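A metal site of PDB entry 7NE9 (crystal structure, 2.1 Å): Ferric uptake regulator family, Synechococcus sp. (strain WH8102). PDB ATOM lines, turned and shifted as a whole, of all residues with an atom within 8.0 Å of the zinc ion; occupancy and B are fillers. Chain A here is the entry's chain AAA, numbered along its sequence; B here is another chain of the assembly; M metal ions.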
ATOM      1  N   THR A  82      12.210  23.186   0.675  1.00  0.00           N
ATOM      2  CA  THR A  82      12.521  24.556   1.140  1.00  0.00           C
ATOM      3  C   THR A  82      13.990  24.581   1.529  1.00  0.00           C
ATOM      4  O   THR A  82      14.425  23.683   2.294  1.00  0.00           O
ATOM      5  CB  THR A  82      11.586  24.969   2.280  1.00  0.00           C
ATOM      6  OG1 THR A  82      10.242  24.869   1.801  1.00  0.00           O
ATOM      7  CG2 THR A  82      11.877  26.377   2.785  1.00  0.00           C
ATOM      8  N   CYS A  83      14.718  25.561   1.020  1.00  0.00           N
ATOM      9  CA  CYS A  83      16.112  25.839   1.446  1.00  0.00           C
ATOM     10  C   CYS A  83      16.092  26.485   2.844  1.00  0.00           C
ATOM     11  O   CYS A  83      15.437  27.501   3.022  1.00  0.00           O
ATOM     12  CB  CYS A  83      16.814  26.737   0.444  1.00  0.00           C
ATOM     13  SG  CYS A  83      18.545  27.019   0.881  1.00  0.00           S
ATOM     14  N   VAL A  84      16.827  25.910   3.784  1.00  0.00           N
ATOM     15  CA  VAL A  84      16.874  26.379   5.201  1.00  0.00           C
ATOM     16  C   VAL A  84      17.732  27.665   5.256  1.00  0.00           C
ATOM     17  O   VAL A  84      17.665  28.361   6.263  1.00  0.00           O
ATOM     18  CB  VAL A  84      17.435  25.298   6.134  1.00  0.00           C
ATOM     19  CG1 VAL A  84      16.541  24.067   6.121  1.00  0.00           C
ATOM     20  CG2 VAL A  84      18.878  24.933   5.815  1.00  0.00           C
ATOM     21  N   ASP A  85      18.550  27.908   4.242  1.00  0.00           N
ATOM     22  CA  ASP A  85      19.479  29.065   4.197  1.00  0.00           C
ATOM     23  C   ASP A  85      18.721  30.278   3.649  1.00  0.00           C
ATOM     24  O   ASP A  85      18.434  31.193   4.443  1.00  0.00           O
ATOM     25  CB  ASP A  85      20.746  28.735   3.408  1.00  0.00           C
ATOM     26  CG  ASP A  85      21.851  29.748   3.627  1.00  0.00           C
ATOM     27  OD1 ASP A  85      21.584  30.786   4.233  1.00  0.00           O
ATOM     28  OD2 ASP A  85      22.976  29.486   3.207  1.00  0.00           O
ATOM     29  N   CYS A  86      18.344  30.269   2.359  1.00  0.00           N
ATOM     30  CA  CYS A  86      17.738  31.422   1.656  1.00  0.00           C
ATOM     31  C   CYS A  86      16.198  31.385   1.708  1.00  0.00           C
ATOM     32  O   CYS A  86      15.594  32.399   1.311  1.00  0.00           O
ATOM     33  CB  CYS A  86      18.247  31.487   0.232  1.00  0.00           C
ATOM     34  SG  CYS A  86      17.585  30.179  -0.852  1.00  0.00           S
ATOM     35  N   GLY A  87      15.565  30.286   2.150  1.00  0.00           N
ATOM     36  CA  GLY A  87      14.090  30.221   2.251  1.00  0.00           C
ATOM     37  C   GLY A  87      13.405  29.981   0.905  1.00  0.00           C
ATOM     38  O   GLY A  87      12.175  29.901   0.892  1.00  0.00           O
ATOM     39  N   THR A  88      14.124  29.821  -0.197  1.00  0.00           N
ATOM     40  CA  THR A  88      13.492  29.503  -1.510  1.00  0.00           C
ATOM     41  C   THR A  88      12.750  28.165  -1.390  1.00  0.00           C
ATOM     42  O   THR A  88      13.248  27.265  -0.703  1.00  0.00           O
ATOM     43  CB  THR A  88      14.520  29.539  -2.652  1.00  0.00           C
ATOM     44  OG1 THR A  88      13.724  29.563  -3.836  1.00  0.00           O
ATOM     45  CG2 THR A  88      15.445  28.346  -2.714  1.00  0.00           C
ATOM     46  N   THR A  89      11.584  28.047  -2.025  1.00  0.00           N
ATOM     47  CA  THR A  89      10.678  26.877  -1.912  1.00  0.00           C
ATOM     48  C   THR A  89      10.219  26.436  -3.294  1.00  0.00           C
ATOM     49  O   THR A  89      10.014  27.296  -4.138  1.00  0.00           O
ATOM     50  CB  THR A  89       9.516  27.194  -0.950  1.00  0.00           C
ATOM     51  OG1 THR A  89       8.877  25.959  -0.594  1.00  0.00           O
ATOM     52  CG2 THR A  89       8.458  28.105  -1.530  1.00  0.00           C
ATOM     53  N   GLY A 121      16.390  21.469   3.093  1.00  0.00           N
ATOM     54  CA  GLY A 121      17.790  21.234   2.728  1.00  0.00           C
ATOM     55  C   GLY A 121      18.432  22.507   2.238  1.00  0.00           C
ATOM     56  O   GLY A 121      17.987  23.605   2.632  1.00  0.00           O
ATOM     57  N   PHE A 122      19.473  22.373   1.421  1.00  0.00           N
ATOM     58  CA  PHE A 122      20.167  23.509   0.774  1.00  0.00           C
ATOM     59  C   PHE A 122      19.893  23.450  -0.723  1.00  0.00           C
ATOM     60  O   PHE A 122      20.071  22.385  -1.312  1.00  0.00           O
ATOM     61  CB  PHE A 122      21.664  23.434   1.034  1.00  0.00           C
ATOM     62  CG  PHE A 122      22.086  23.528   2.473  1.00  0.00           C
ATOM     63  CD1 PHE A 122      21.827  24.668   3.226  1.00  0.00           C
ATOM     64  CD2 PHE A 122      22.800  22.489   3.071  1.00  0.00           C
ATOM     65  CE1 PHE A 122      22.237  24.747   4.552  1.00  0.00           C
ATOM     66  CE2 PHE A 122      23.230  22.581   4.388  1.00  0.00           C
ATOM     67  CZ  PHE A 122      22.934  23.699   5.122  1.00  0.00           C
ATOM     68  N   CYS A 123      19.475  24.579  -1.292  1.00  0.00           N
ATOM     69  CA  CYS A 123      19.356  24.751  -2.766  1.00  0.00           C
ATOM     70  C   CYS A 123      20.767  24.824  -3.380  1.00  0.00           C
ATOM     71  O   CYS A 123      21.756  24.902  -2.633  1.00  0.00           O
ATOM     72  CB  CYS A 123      18.522  25.984  -3.076  1.00  0.00           C
ATOM     73  SG  CYS A 123      19.428  27.535  -2.848  1.00  0.00           S
ATOM     74  N   SER A 124      20.843  24.801  -4.722  1.00  0.00           N
ATOM     75  CA  SER A 124      22.090  24.844  -5.546  1.00  0.00           C
ATOM     76  C   SER A 124      23.013  25.969  -5.086  1.00  0.00           C
ATOM     77  O   SER A 124      24.200  25.712  -4.865  1.00  0.00           O
ATOM     78  CB  SER A 124      21.765  25.011  -7.019  1.00  0.00           C
ATOM     79  OG  SER A 124      20.969  23.947  -7.511  1.00  0.00           O
ATOM     80  N   SER A 125      22.464  27.187  -4.966  1.00  0.00           N
ATOM     81  CA  SER A 125      23.207  28.414  -4.573  1.00  0.00           C
ATOM     82  C   SER A 125      23.821  28.273  -3.175  1.00  0.00           C
ATOM     83  O   SER A 125      24.906  28.823  -2.964  1.00  0.00           O
ATOM     84  CB  SER A 125      22.324  29.627  -4.629  1.00  0.00           C
ATOM     85  OG  SER A 125      21.546  29.621  -5.802  1.00  0.00           O
ATOM     86  N   CYS A 126      23.152  27.593  -2.237  1.00  0.00           N
ATOM     87  CA  CYS A 126      23.485  27.649  -0.782  1.00  0.00           C
ATOM     88  C   CYS A 126      24.350  26.451  -0.353  1.00  0.00           C
ATOM     89  O   CYS A 126      24.946  26.550   0.725  1.00  0.00           O
ATOM     90  CB  CYS A 126      22.212  27.693   0.071  1.00  0.00           C
ATOM     91  SG  CYS A 126      21.277  29.241  -0.090  1.00  0.00           S
ATOM     92  N   ARG A 127      24.419  25.358  -1.124  1.00  0.00           N
ATOM     93  CA  ARG A 127      24.955  24.053  -0.649  1.00  0.00           C
ATOM     94  C   ARG A 127      26.469  24.133  -0.447  1.00  0.00           C
ATOM     95  O   ARG A 127      27.181  24.474  -1.379  1.00  0.00           O
ATOM     96  CB  ARG A 127      24.620  22.912  -1.619  1.00  0.00           C
ATOM     97  CG  ARG A 127      24.828  23.288  -3.076  1.00  0.00           C
ATOM     98  CD  ARG A 127      25.085  22.129  -4.001  1.00  0.00           C
ATOM     99  NE  ARG A 127      23.815  21.548  -4.428  1.00  0.00           N
ATOM    100  CZ  ARG A 127      23.428  20.274  -4.273  1.00  0.00           C
ATOM    101  NH1 ARG A 127      24.227  19.394  -3.691  1.00  0.00           N
ATOM    102  NH2 ARG A 127      22.246  19.902  -4.721  1.00  0.00           N
ATOM    103  N   PHE B 110      19.013  19.664  -5.412  1.00  0.00           N
ATOM    104  CA  PHE B 110      18.717  20.213  -4.066  1.00  0.00           C
ATOM    105  C   PHE B 110      19.328  19.242  -3.054  1.00  0.00           C
ATOM    106  O   PHE B 110      19.100  18.030  -3.228  1.00  0.00           O
ATOM    107  CB  PHE B 110      17.190  20.273  -3.953  1.00  0.00           C
ATOM    108  CG  PHE B 110      16.679  20.891  -2.693  1.00  0.00           C
ATOM    109  CD1 PHE B 110      16.491  22.269  -2.613  1.00  0.00           C
ATOM    110  CD2 PHE B 110      16.379  20.108  -1.589  1.00  0.00           C
ATOM    111  CE1 PHE B 110      16.013  22.856  -1.459  1.00  0.00           C
ATOM    112  CE2 PHE B 110      15.895  20.694  -0.426  1.00  0.00           C
ATOM    113  CZ  PHE B 110      15.712  22.063  -0.369  1.00  0.00           C
HETATM  114 ZN    ZN M   1      19.167  28.524  -0.792  1.00  0.00          ZN
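SG of Cys 86 lies close to N of Thr 88. SG of Cys 123 lies close to N of Ser 125, at 3.7 Å. O of Thr 88 lies within hydrogen-bond range of N of Cys 83, 2.8 Å away. The side-chain sulfur of Cys 83 sits close to the backbone NH of Asp 85 (3.5 Å). The side-chain sulfur (SG) of Cys 126 sits close to the side-chain carboxylate (OD2) of Asp 85 (3.7 Å).
Within 4 Å of the zinc ion: Cys 83, Cys 86, Cys 123 and Cys 126. The nearest printed residue that does not touch the zinc ion is Thr 88 (4.2 Å).
The zinc ion is bound by SG of Cys 86 (2.3 Å), SG of Cys 123 (2.3 Å), SG of Cys 83 (2.3 Å) and SG of Cys 126 (2.3 Å).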
